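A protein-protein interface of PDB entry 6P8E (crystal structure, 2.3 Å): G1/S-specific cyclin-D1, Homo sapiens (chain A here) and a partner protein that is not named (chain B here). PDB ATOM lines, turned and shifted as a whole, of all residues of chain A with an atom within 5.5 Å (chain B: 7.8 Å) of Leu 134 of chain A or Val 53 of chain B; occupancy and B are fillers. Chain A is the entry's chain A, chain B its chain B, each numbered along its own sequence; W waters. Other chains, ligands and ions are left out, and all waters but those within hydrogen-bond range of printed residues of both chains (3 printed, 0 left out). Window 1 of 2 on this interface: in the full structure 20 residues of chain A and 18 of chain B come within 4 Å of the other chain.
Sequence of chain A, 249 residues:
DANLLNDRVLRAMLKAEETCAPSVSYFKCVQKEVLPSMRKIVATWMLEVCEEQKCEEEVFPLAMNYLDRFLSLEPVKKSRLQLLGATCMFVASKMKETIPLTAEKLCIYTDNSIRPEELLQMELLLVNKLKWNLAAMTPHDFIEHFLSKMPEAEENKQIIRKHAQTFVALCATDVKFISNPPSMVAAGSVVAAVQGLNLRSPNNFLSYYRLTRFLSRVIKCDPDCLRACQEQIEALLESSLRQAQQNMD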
ATOM      1  N   CYS A  20      17.181 -16.473 -17.930  1.00  0.00           N
ATOM      2  CA  CYS A  20      18.533 -17.027 -17.883  1.00  0.00           C
ATOM      3  C   CYS A  20      18.724 -18.094 -18.951  1.00  0.00           C
ATOM      4  O   CYS A  20      19.382 -19.102 -18.728  1.00  0.00           O
ATOM      5  CB  CYS A  20      18.856 -17.599 -16.500  1.00  0.00           C
ATOM      6  SG  CYS A  20      19.179 -16.357 -15.151  1.00  0.00           S
ATOM      7  N   LEU A  62      23.840 -26.130 -13.326  1.00  0.00           N
ATOM      8  CA  LEU A  62      23.937 -24.678 -13.214  1.00  0.00           C
ATOM      9  C   LEU A  62      25.175 -24.170 -13.952  1.00  0.00           C
ATOM     10  O   LEU A  62      25.133 -23.122 -14.607  1.00  0.00           O
ATOM     11  CB  LEU A  62      23.947 -24.260 -11.736  1.00  0.00           C
ATOM     12  CG  LEU A  62      24.021 -22.753 -11.442  1.00  0.00           C
ATOM     13  CD1 LEU A  62      22.846 -21.983 -12.126  1.00  0.00           C
ATOM     14  CD2 LEU A  62      24.073 -22.421  -9.934  1.00  0.00           C
ATOM     15  N   TYR A  66      25.584 -21.516 -17.207  1.00  0.00           N
ATOM     16  CA  TYR A  66      26.525 -20.408 -17.331  1.00  0.00           C
ATOM     17  C   TYR A  66      27.332 -20.537 -18.609  1.00  0.00           C
ATOM     18  O   TYR A  66      27.584 -19.537 -19.310  1.00  0.00           O
ATOM     19  CB  TYR A  66      27.477 -20.372 -16.141  1.00  0.00           C
ATOM     20  CG  TYR A  66      26.869 -20.092 -14.791  1.00  0.00           C
ATOM     21  CD1 TYR A  66      27.574 -20.419 -13.621  1.00  0.00           C
ATOM     22  CD2 TYR A  66      25.619 -19.490 -14.667  1.00  0.00           C
ATOM     23  CE1 TYR A  66      27.038 -20.146 -12.354  1.00  0.00           C
ATOM     24  CE2 TYR A  66      25.062 -19.230 -13.420  1.00  0.00           C
ATOM     25  CZ  TYR A  66      25.784 -19.552 -12.262  1.00  0.00           C
ATOM     26  OH  TYR A  66      25.241 -19.289 -11.032  1.00  0.00           O
ATOM     27  N   ARG A  69      25.260 -19.799 -21.732  1.00  0.00           N
ATOM     28  CA  ARG A  69      24.978 -18.364 -21.791  1.00  0.00           C
ATOM     29  C   ARG A  69      26.204 -17.566 -22.206  1.00  0.00           C
ATOM     30  O   ARG A  69      26.095 -16.640 -23.010  1.00  0.00           O
ATOM     31  CB  ARG A  69      24.452 -17.863 -20.452  1.00  0.00           C
ATOM     32  CG  ARG A  69      23.003 -18.214 -20.248  1.00  0.00           C
ATOM     33  CD  ARG A  69      22.351 -17.260 -19.310  1.00  0.00           C
ATOM     34  NE  ARG A  69      22.517 -17.750 -17.961  1.00  0.00           N
ATOM     35  CZ  ARG A  69      22.585 -16.979 -16.887  1.00  0.00           C
ATOM     36  NH1 ARG A  69      22.491 -15.659 -16.994  1.00  0.00           N
ATOM     37  NH2 ARG A  69      22.725 -17.543 -15.702  1.00  0.00           N
ATOM     38  N   VAL A  91      31.913 -20.741 -10.067  1.00  0.00           N
ATOM     39  CA  VAL A  91      30.823 -19.848  -9.678  1.00  0.00           C
ATOM     40  C   VAL A  91      29.591 -20.650  -9.265  1.00  0.00           C
ATOM     41  O   VAL A  91      28.911 -20.304  -8.298  1.00  0.00           O
ATOM     42  CB  VAL A  91      30.499 -18.874 -10.834  1.00  0.00           C
ATOM     43  CG1 VAL A  91      29.265 -18.019 -10.494  1.00  0.00           C
ATOM     44  CG2 VAL A  91      31.706 -18.009 -11.146  1.00  0.00           C
ATOM     45  N   LYS A  94      29.909 -21.799  -5.743  1.00  0.00           N
ATOM     46  CA  LYS A  94      29.682 -20.751  -4.759  1.00  0.00           C
ATOM     47  C   LYS A  94      28.204 -20.492  -4.564  1.00  0.00           C
ATOM     48  O   LYS A  94      27.759 -20.203  -3.448  1.00  0.00           O
ATOM     49  CB  LYS A  94      30.384 -19.476  -5.194  1.00  0.00           C
ATOM     50  CG  LYS A  94      31.899 -19.590  -5.146  1.00  0.00           C
ATOM     51  CD  LYS A  94      32.522 -18.254  -5.467  1.00  0.00           C
ATOM     52  CE  LYS A  94      33.971 -18.366  -5.831  1.00  0.00           C
ATOM     53  NZ  LYS A  94      34.614 -17.002  -5.800  1.00  0.00           N
ATOM     54  N   MET A  95      27.423 -20.580  -5.647  1.00  0.00           N
ATOM     55  CA  MET A  95      25.993 -20.358  -5.532  1.00  0.00           C
ATOM     56  C   MET A  95      25.297 -21.483  -4.775  1.00  0.00           C
ATOM     57  O   MET A  95      24.304 -21.234  -4.099  1.00  0.00           O
ATOM     58  CB  MET A  95      25.388 -20.183  -6.923  1.00  0.00           C
ATOM     59  CG  MET A  95      25.951 -18.971  -7.643  1.00  0.00           C
ATOM     60  SD  MET A  95      25.409 -17.427  -6.820  1.00  0.00           S
ATOM     61  CE  MET A  95      23.645 -17.509  -7.144  1.00  0.00           C
ATOM     62  N   GLU A 123      36.624 -15.509 -13.737  1.00  0.00           N
ATOM     63  CA  GLU A 123      35.395 -15.425 -12.955  1.00  0.00           C
ATOM     64  C   GLU A 123      34.804 -14.028 -13.044  1.00  0.00           C
ATOM     65  O   GLU A 123      33.586 -13.871 -13.147  1.00  0.00           O
ATOM     66  CB  GLU A 123      35.651 -15.813 -11.497  1.00  0.00           C
ATOM     67  CG  GLU A 123      34.494 -15.489 -10.563  1.00  0.00           C
ATOM     68  CD  GLU A 123      34.799 -15.757  -9.083  1.00  0.00           C
ATOM     69  OE1 GLU A 123      35.834 -15.275  -8.571  1.00  0.00           O
ATOM     70  OE2 GLU A 123      33.996 -16.452  -8.427  1.00  0.00           O
ATOM     71  N   VAL A 127      31.118 -13.487 -14.716  1.00  0.00           N
ATOM     72  CA  VAL A 127      30.064 -12.893 -13.901  1.00  0.00           C
ATOM     73  C   VAL A 127      29.610 -11.564 -14.490  1.00  0.00           C
ATOM     74  O   VAL A 127      28.411 -11.261 -14.514  1.00  0.00           O
ATOM     75  CB  VAL A 127      30.552 -12.724 -12.458  1.00  0.00           C
ATOM     76  CG1 VAL A 127      29.541 -11.965 -11.676  1.00  0.00           C
ATOM     77  CG2 VAL A 127      30.813 -14.099 -11.827  1.00  0.00           C
ATOM     78  N   LEU A 130      27.557 -12.090 -17.695  1.00  0.00           N
ATOM     79  CA  LEU A 130      26.192 -12.468 -17.375  1.00  0.00           C
ATOM     80  C   LEU A 130      25.427 -11.362 -16.633  1.00  0.00           C
ATOM     81  O   LEU A 130      24.286 -11.593 -16.227  1.00  0.00           O
ATOM     82  CB  LEU A 130      26.187 -13.758 -16.542  1.00  0.00           C
ATOM     83  CG  LEU A 130      26.855 -14.996 -17.155  1.00  0.00           C
ATOM     84  CD1 LEU A 130      26.597 -16.249 -16.306  1.00  0.00           C
ATOM     85  CD2 LEU A 130      26.410 -15.219 -18.576  1.00  0.00           C
ATOM     86  N   TRP A 132      25.638 -10.524 -13.773  1.00  0.00           N
ATOM     87  CA  TRP A 132      25.383 -11.074 -12.451  1.00  0.00           C
ATOM     88  C   TRP A 132      24.038 -11.785 -12.362  1.00  0.00           C
ATOM     89  O   TRP A 132      23.501 -11.961 -11.260  1.00  0.00           O
ATOM     90  CB  TRP A 132      25.479 -10.001 -11.364  1.00  0.00           C
ATOM     91  CG  TRP A 132      26.818  -9.385 -11.269  1.00  0.00           C
ATOM     92  CD1 TRP A 132      27.408  -8.560 -12.182  1.00  0.00           C
ATOM     93  CD2 TRP A 132      27.750  -9.523 -10.187  1.00  0.00           C
ATOM     94  NE1 TRP A 132      28.657  -8.189 -11.744  1.00  0.00           N
ATOM     95  CE2 TRP A 132      28.889  -8.764 -10.520  1.00  0.00           C
ATOM     96  CE3 TRP A 132      27.732 -10.223  -8.979  1.00  0.00           C
ATOM     97  CZ2 TRP A 132      29.999  -8.666  -9.675  1.00  0.00           C
ATOM     98  CZ3 TRP A 132      28.829 -10.135  -8.148  1.00  0.00           C
ATOM     99  CH2 TRP A 132      29.954  -9.363  -8.504  1.00  0.00           C
ATOM    100  N   ASN A 133      23.483 -12.231 -13.490  1.00  0.00           N
ATOM    101  CA  ASN A 133      22.304 -13.090 -13.422  1.00  0.00           C
ATOM    102  C   ASN A 133      22.768 -14.520 -13.160  1.00  0.00           C
ATOM    103  O   ASN A 133      22.776 -15.383 -14.044  1.00  0.00           O
ATOM    104  CB  ASN A 133      21.479 -12.986 -14.693  1.00  0.00           C
ATOM    105  CG  ASN A 133      20.864 -11.620 -14.854  1.00  0.00           C
ATOM    106  OD1 ASN A 133      19.912 -11.271 -14.161  1.00  0.00           O
ATOM    107  ND2 ASN A 133      21.411 -10.831 -15.766  1.00  0.00           N
ATOM    108  N   LEU A 134      23.139 -14.781 -11.902  1.00  0.00           N
ATOM    109  CA  LEU A 134      23.678 -16.078 -11.519  1.00  0.00           C
ATOM    110  C   LEU A 134      22.651 -16.998 -10.886  1.00  0.00           C
ATOM    111  O   LEU A 134      22.895 -18.221 -10.795  1.00  0.00           O
ATOM    112  CB  LEU A 134      24.851 -15.894 -10.546  1.00  0.00           C
ATOM    113  CG  LEU A 134      25.892 -14.837 -10.916  1.00  0.00           C
ATOM    114  CD1 LEU A 134      27.026 -14.881  -9.902  1.00  0.00           C
ATOM    115  CD2 LEU A 134      26.411 -15.109 -12.318  1.00  0.00           C
ATOM    116  N   ALA A 135      21.539 -16.446 -10.419  1.00  0.00           N
ATOM    117  CA  ALA A 135      20.527 -17.221  -9.704  1.00  0.00           C
ATOM    118  C   ALA A 135      19.538 -17.863 -10.677  1.00  0.00           C
ATOM    119  O   ALA A 135      18.335 -17.695 -10.554  1.00  0.00           O
ATOM    120  CB  ALA A 135      19.810 -16.332  -8.691  1.00  0.00           C
ATOM    121  N   ALA A 136      20.043 -18.609 -11.658  1.00  0.00           N
ATOM    122  CA  ALA A 136      19.165 -19.183 -12.674  1.00  0.00           C
ATOM    123  C   ALA A 136      18.348 -20.320 -12.085  1.00  0.00           C
ATOM    124  O   ALA A 136      18.812 -21.033 -11.194  1.00  0.00           O
ATOM    125  CB  ALA A 136      19.984 -19.696 -13.860  1.00  0.00           C
ATOM    126  N   GLY B  47      38.762 -15.533  -4.855  1.00  0.00           N
ATOM    127  CA  GLY B  47      38.031 -14.629  -5.733  1.00  0.00           C
ATOM    128  C   GLY B  47      36.862 -13.955  -5.046  1.00  0.00           C
ATOM    129  O   GLY B  47      36.921 -13.601  -3.864  1.00  0.00           O
ATOM    130  N   LEU B  48      35.781 -13.781  -5.797  1.00  0.00           N
ATOM    131  CA  LEU B  48      34.609 -13.100  -5.268  1.00  0.00           C
ATOM    132  C   LEU B  48      34.066 -13.836  -4.049  1.00  0.00           C
ATOM    133  O   LEU B  48      33.931 -15.072  -4.080  1.00  0.00           O
ATOM    134  CB  LEU B  48      33.517 -12.986  -6.330  1.00  0.00           C
ATOM    135  CG  LEU B  48      33.781 -12.084  -7.533  1.00  0.00           C
ATOM    136  CD1 LEU B  48      32.660 -12.246  -8.546  1.00  0.00           C
ATOM    137  CD2 LEU B  48      33.942 -10.625  -7.124  1.00  0.00           C
ATOM    138  N   PRO B  49      33.732 -13.125  -2.971  1.00  0.00           N
ATOM    139  CA  PRO B  49      33.183 -13.795  -1.789  1.00  0.00           C
ATOM    140  C   PRO B  49      31.832 -14.426  -2.095  1.00  0.00           C
ATOM    141  O   PRO B  49      31.081 -13.959  -2.952  1.00  0.00           O
ATOM    142  CB  PRO B  49      33.056 -12.661  -0.763  1.00  0.00           C
ATOM    143  CG  PRO B  49      33.981 -11.581  -1.281  1.00  0.00           C
ATOM    144  CD  PRO B  49      33.894 -11.678  -2.763  1.00  0.00           C
ATOM    145  N   ILE B  50      31.545 -15.523  -1.393  1.00  0.00           N
ATOM    146  CA  ILE B  50      30.280 -16.225  -1.584  1.00  0.00           C
ATOM    147  C   ILE B  50      29.109 -15.274  -1.380  1.00  0.00           C
ATOM    148  O   ILE B  50      28.199 -15.187  -2.214  1.00  0.00           O
ATOM    149  CB  ILE B  50      30.190 -17.433  -0.636  1.00  0.00           C
ATOM    150  CG1 ILE B  50      31.184 -18.515  -1.064  1.00  0.00           C
ATOM    151  CG2 ILE B  50      28.760 -17.972  -0.582  1.00  0.00           C
ATOM    152  CD1 ILE B  50      31.740 -19.285   0.086  1.00  0.00           C
ATOM    153  N   SER B  51      29.112 -14.551  -0.259  1.00  0.00           N
ATOM    154  CA  SER B  51      27.991 -13.670   0.046  1.00  0.00           C
ATOM    155  C   SER B  51      27.808 -12.595  -1.024  1.00  0.00           C
ATOM    156  O   SER B  51      26.681 -12.145  -1.263  1.00  0.00           O
ATOM    157  CB  SER B  51      28.191 -13.028   1.411  1.00  0.00           C
ATOM    158  OG  SER B  51      29.297 -12.140   1.366  1.00  0.00           O
ATOM    159  N   THR B  52      28.889 -12.179  -1.690  1.00  0.00           N
ATOM    160  CA  THR B  52      28.746 -11.156  -2.717  1.00  0.00           C
ATOM    161  C   THR B  52      28.033 -11.693  -3.951  1.00  0.00           C
ATOM    162  O   THR B  52      27.102 -11.051  -4.454  1.00  0.00           O
ATOM    163  CB  THR B  52      30.096 -10.564  -3.114  1.00  0.00           C
ATOM    164  OG1 THR B  52      30.754 -10.029  -1.959  1.00  0.00           O
ATOM    165  CG2 THR B  52      29.867  -9.434  -4.106  1.00  0.00           C
ATOM    166  N   VAL B  53      28.459 -12.852  -4.473  1.00  0.00           N
ATOM    167  CA  VAL B  53      27.817 -13.357  -5.686  1.00  0.00           C
ATOM    168  C   VAL B  53      26.373 -13.746  -5.403  1.00  0.00           C
ATOM    169  O   VAL B  53      25.495 -13.514  -6.238  1.00  0.00           O
ATOM    170  CB  VAL B  53      28.595 -14.525  -6.339  1.00  0.00           C
ATOM    171  CG1 VAL B  53      29.994 -14.103  -6.668  1.00  0.00           C
ATOM    172  CG2 VAL B  53      28.589 -15.765  -5.466  1.00  0.00           C
ATOM    173  N   ARG B  54      26.090 -14.322  -4.231  1.00  0.00           N
ATOM    174  CA  ARG B  54      24.709 -14.712  -3.939  1.00  0.00           C
ATOM    175  C   ARG B  54      23.807 -13.485  -3.756  1.00  0.00           C
ATOM    176  O   ARG B  54      22.715 -13.411  -4.327  1.00  0.00           O
ATOM    177  CB  ARG B  54      24.655 -15.593  -2.691  1.00  0.00           C
ATOM    178  CG  ARG B  54      25.297 -16.957  -2.883  1.00  0.00           C
ATOM    179  CD  ARG B  54      25.072 -17.839  -1.654  1.00  0.00           C
ATOM    180  NE  ARG B  54      25.753 -19.098  -1.835  1.00  0.00           N
ATOM    181  CZ  ARG B  54      25.887 -20.020  -0.894  1.00  0.00           C
ATOM    182  NH1 ARG B  54      25.370 -19.798   0.295  1.00  0.00           N
ATOM    183  NH2 ARG B  54      26.552 -21.152  -1.155  1.00  0.00           N
ATOM    184  N   GLU B  55      24.247 -12.507  -2.966  1.00  0.00           N
ATOM    185  CA  GLU B  55      23.365 -11.387  -2.666  1.00  0.00           C
ATOM    186  C   GLU B  55      23.121 -10.522  -3.903  1.00  0.00           C
ATOM    187  O   GLU B  55      21.980 -10.156  -4.187  1.00  0.00           O
ATOM    188  CB  GLU B  55      23.932 -10.573  -1.510  1.00  0.00           C
ATOM    189  CG  GLU B  55      23.222 -10.854  -0.181  1.00  0.00           C
ATOM    190  CD  GLU B  55      21.693 -10.621  -0.224  1.00  0.00           C
ATOM    191  OE1 GLU B  55      20.979 -11.191   0.634  1.00  0.00           O
ATOM    192  OE2 GLU B  55      21.201  -9.866  -1.099  1.00  0.00           O
ATOM    193  N   VAL B  56      24.168 -10.222  -4.676  1.00  0.00           N
ATOM    194  CA  VAL B  56      23.967  -9.456  -5.899  1.00  0.00           C
ATOM    195  C   VAL B  56      23.097 -10.226  -6.889  1.00  0.00           C
ATOM    196  O   VAL B  56      22.206  -9.644  -7.517  1.00  0.00           O
ATOM    197  CB  VAL B  56      25.309  -9.039  -6.520  1.00  0.00           C
ATOM    198  CG1 VAL B  56      25.042  -8.290  -7.815  1.00  0.00           C
ATOM    199  CG2 VAL B  56      26.104  -8.145  -5.525  1.00  0.00           C
ATOM    200  N   ALA B  57      23.303 -11.549  -7.019  1.00  0.00           N
ATOM    201  CA  ALA B  57      22.474 -12.326  -7.942  1.00  0.00           C
ATOM    202  C   ALA B  57      21.001 -12.339  -7.513  1.00  0.00           C
ATOM    203  O   ALA B  57      20.099 -12.316  -8.361  1.00  0.00           O
ATOM    204  CB  ALA B  57      22.998 -13.751  -8.061  1.00  0.00           C
ATOM    205  N   LEU B  58      20.736 -12.400  -6.207  1.00  0.00           N
ATOM    206  CA  LEU B  58      19.358 -12.293  -5.734  1.00  0.00           C
ATOM    207  C   LEU B  58      18.702 -10.965  -6.163  1.00  0.00           C
ATOM    208  O   LEU B  58      17.532 -10.946  -6.565  1.00  0.00           O
ATOM    209  CB  LEU B  58      19.330 -12.467  -4.219  1.00  0.00           C
ATOM    210  CG  LEU B  58      17.970 -12.163  -3.585  1.00  0.00           C
ATOM    211  CD1 LEU B  58      16.941 -13.213  -3.970  1.00  0.00           C
ATOM    212  CD2 LEU B  58      18.090 -12.065  -2.075  1.00  0.00           C
ATOM    213  N   LEU B  59      19.439  -9.850  -6.109  1.00  0.00           N
ATOM    214  CA  LEU B  59      18.884  -8.578  -6.583  1.00  0.00           C
ATOM    215  C   LEU B  59      18.620  -8.608  -8.080  1.00  0.00           C
ATOM    216  O   LEU B  59      17.662  -7.992  -8.564  1.00  0.00           O
ATOM    217  CB  LEU B  59      19.826  -7.414  -6.281  1.00  0.00           C
ATOM    218  CG  LEU B  59      20.208  -7.118  -4.837  1.00  0.00           C
ATOM    219  CD1 LEU B  59      21.066  -5.871  -4.834  1.00  0.00           C
ATOM    220  CD2 LEU B  59      18.982  -6.941  -3.950  1.00  0.00           C
ATOM    221  N   ARG B  60      19.492  -9.273  -8.834  1.00  0.00           N
ATOM    222  CA  ARG B  60      19.271  -9.397 -10.265  1.00  0.00           C
ATOM    223  C   ARG B  60      18.027 -10.220 -10.550  1.00  0.00           C
ATOM    224  O   ARG B  60      17.279  -9.912 -11.479  1.00  0.00           O
ATOM    225  CB  ARG B  60      20.490 -10.032 -10.935  1.00  0.00           C
ATOM    226  CG  ARG B  60      21.498  -9.031 -11.412  1.00  0.00           C
ATOM    227  CD  ARG B  60      20.898  -8.170 -12.491  1.00  0.00           C
ATOM    228  NE  ARG B  60      21.912  -7.355 -13.132  1.00  0.00           N
ATOM    229  CZ  ARG B  60      21.665  -6.206 -13.741  1.00  0.00           C
ATOM    230  NH1 ARG B  60      20.423  -5.730 -13.781  1.00  0.00           N
ATOM    231  NH2 ARG B  60      22.665  -5.531 -14.296  1.00  0.00           N
ATOM    232  N   ARG B  61      17.800 -11.282  -9.768  1.00  0.00           N
ATOM    233  CA  ARG B  61      16.632 -12.137  -9.982  1.00  0.00           C
ATOM    234  C   ARG B  61      15.336 -11.377  -9.688  1.00  0.00           C
ATOM    235  O   ARG B  61      14.373 -11.454 -10.463  1.00  0.00           O
ATOM    236  CB  ARG B  61      16.733 -13.392  -9.105  1.00  0.00           C
ATOM    237  CG  ARG B  61      15.700 -14.474  -9.416  1.00  0.00           C
ATOM    238  CD  ARG B  61      15.961 -15.756  -8.634  1.00  0.00           C
ATOM    239  NE  ARG B  61      15.789 -15.558  -7.199  1.00  0.00           N
ATOM    240  CZ  ARG B  61      14.626 -15.701  -6.569  1.00  0.00           C
ATOM    241  NH1 ARG B  61      13.538 -16.045  -7.256  1.00  0.00           N
ATOM    242  NH2 ARG B  61      14.546 -15.506  -5.255  1.00  0.00           N
ATOM    243  N   VAL B  88      32.387  -3.169  -5.868  1.00  0.00           N
ATOM    244  CA  VAL B  88      31.091  -3.411  -6.493  1.00  0.00           C
ATOM    245  C   VAL B  88      30.213  -2.186  -6.285  1.00  0.00           C
ATOM    246  O   VAL B  88      29.957  -1.783  -5.144  1.00  0.00           O
ATOM    247  CB  VAL B  88      30.412  -4.670  -5.934  1.00  0.00           C
ATOM    248  CG1 VAL B  88      29.077  -4.861  -6.590  1.00  0.00           C
ATOM    249  CG2 VAL B  88      31.284  -5.890  -6.172  1.00  0.00           C
HETATM  250  O   HOH W   1      17.393  -9.905 -14.239  1.00  0.00           O
HETATM  251  O   HOH W   2      34.954 -16.963  -2.330  1.00  0.00           O
HETATM  252  O   HOH W   3      20.363 -13.768 -10.577  1.00  0.00           O
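Leu 134 of chain A touches just these residues of chain B: Val 53 (3.9 Å) and Ala 57 (3.8 Å). Of chain A, only Met 95 and Leu 134 come within 4 Å of Val 53 of chain B. Printed residues of chain B within 4 Å of Met 95 of chain A: Val 53 (3.8 Å), Arg 54 (3.4 Å) and Ala 57 (3.9 Å). Of the printed residues of chain A, Ile 50 of chain B touches Lys 94 (3.8 Å). Ser 51 of chain B touches none of the printed residues of chain A. Leu 62 of chain A touches none of the printed residues of chain B. The nearest residue of chain B that does not touch Leu 134 of chain A is Arg 60 of chain B (5.5 Å). The nearest residue of chain A that does not touch Val 53 of chain B is Lys 94 of chain A (4.1 Å).
Water W3 lies within hydrogen-bond range of O of Ala 57 of chain B (2.7 Å), N of Ala 135 of chain A (2.9 Å) and N of Leu 134 of chain A (3.2 Å). Water W1 bridges O of Arg 60 of chain B (2.8 Å) and OD1 of Asn 133 of chain A (2.9 Å). Water W2 lies within hydrogen-bond range of O of Leu 48 of chain B and NZ of Lys 94 of chain A.
The side-chain hydroxyl (OH) of Tyr 66 of chain A lies within hydrogen-bond range of the backbone carbonyl oxygen (O) of Leu 134 of chain A, at 2.6 Å. O of Asn 133 of chain A sits at hydrogen-bond distance from NH2 of Arg 69 of chain A (2.7 Å). The side-chain amino group (NZ) of Lys 94 of chain A is in salt-bridge range of the side-chain carboxylate (OE2) of Glu 123 of chain A, at 2.8 Å. The backbone NH (N) of Trp 132 of chain A sits at hydrogen-bond distance from the backbone carbonyl oxygen (O) of Val 127 of chain A, 3.0 Å away. O of Leu 130 of chain A sits at hydrogen-bond distance from ND2 of Asn 133 of chain A (3.0 Å).
O of Leu 48 of chain B is in hydrogen-bond range of NZ of Lys 94 of chain A (2.7 Å). The backbone carbonyl oxygen of Lys 94 of chain A is in hydrogen-bond range of the guanidinium group of Arg 54 of chain B. The backbone carbonyl oxygen (O) of Met 95 of chain A sits at hydrogen-bond distance from the guanidinium group (NE) of Arg 54 of chain B (3.4 Å). OE1 of Glu 123 of chain A lies within hydrogen-bond range of N of Leu 48 of chain B, at 3.2 Å.
Among the printed residues, pairs that only touch across the chains: Lys 94 of chain A with Gly 47 of chain B (3.9 Å), Lys 94 of chain A with Ile 50 of chain B (3.8 Å), Met 95 of chain A with Val 53 of chain B (3.8 Å), Met 95 of chain A with Ala 57 of chain B (3.9 Å), Glu 123 of chain A with Gly 47 of chain B (3.6 Å), Trp 132 of chain A with Leu 48 of chain B (3.95 Å), Trp 132 of chain A with Val 56 of chain B (3.5 Å), Trp 132 of chain A with Ala 57 of chain B (3.5 Å), Trp 132 of chain A with Arg 60 of chain B (3.6 Å), Asn 133 of chain A with Arg 60 of chain B (3.5 Å), Leu 134 of chain A with Val 53 of chain B (3.9 Å), Leu 134 of chain A with Ala 57 of chain B (3.8 Å), Ala 135 of chain A with Ala 57 of chain B (3.9 Å) and Ala 135 of chain A with Arg 61 of chain B (3.6 Å).
Of the 15 printed residues of chain A, 7 touch a printed residue of chain B. Printed residues of chain A that touch a printed residue of chain B: Lys 94, Met 95, Glu 123, Trp 132, Asn 133, Leu 134 and Ala 135. Printed residues of chain B that touch a printed residue of chain A: Gly 47, Leu 48, Ile 50, Val 53, Arg 54, Val 56, Ala 57, Arg 60 and Arg 61.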
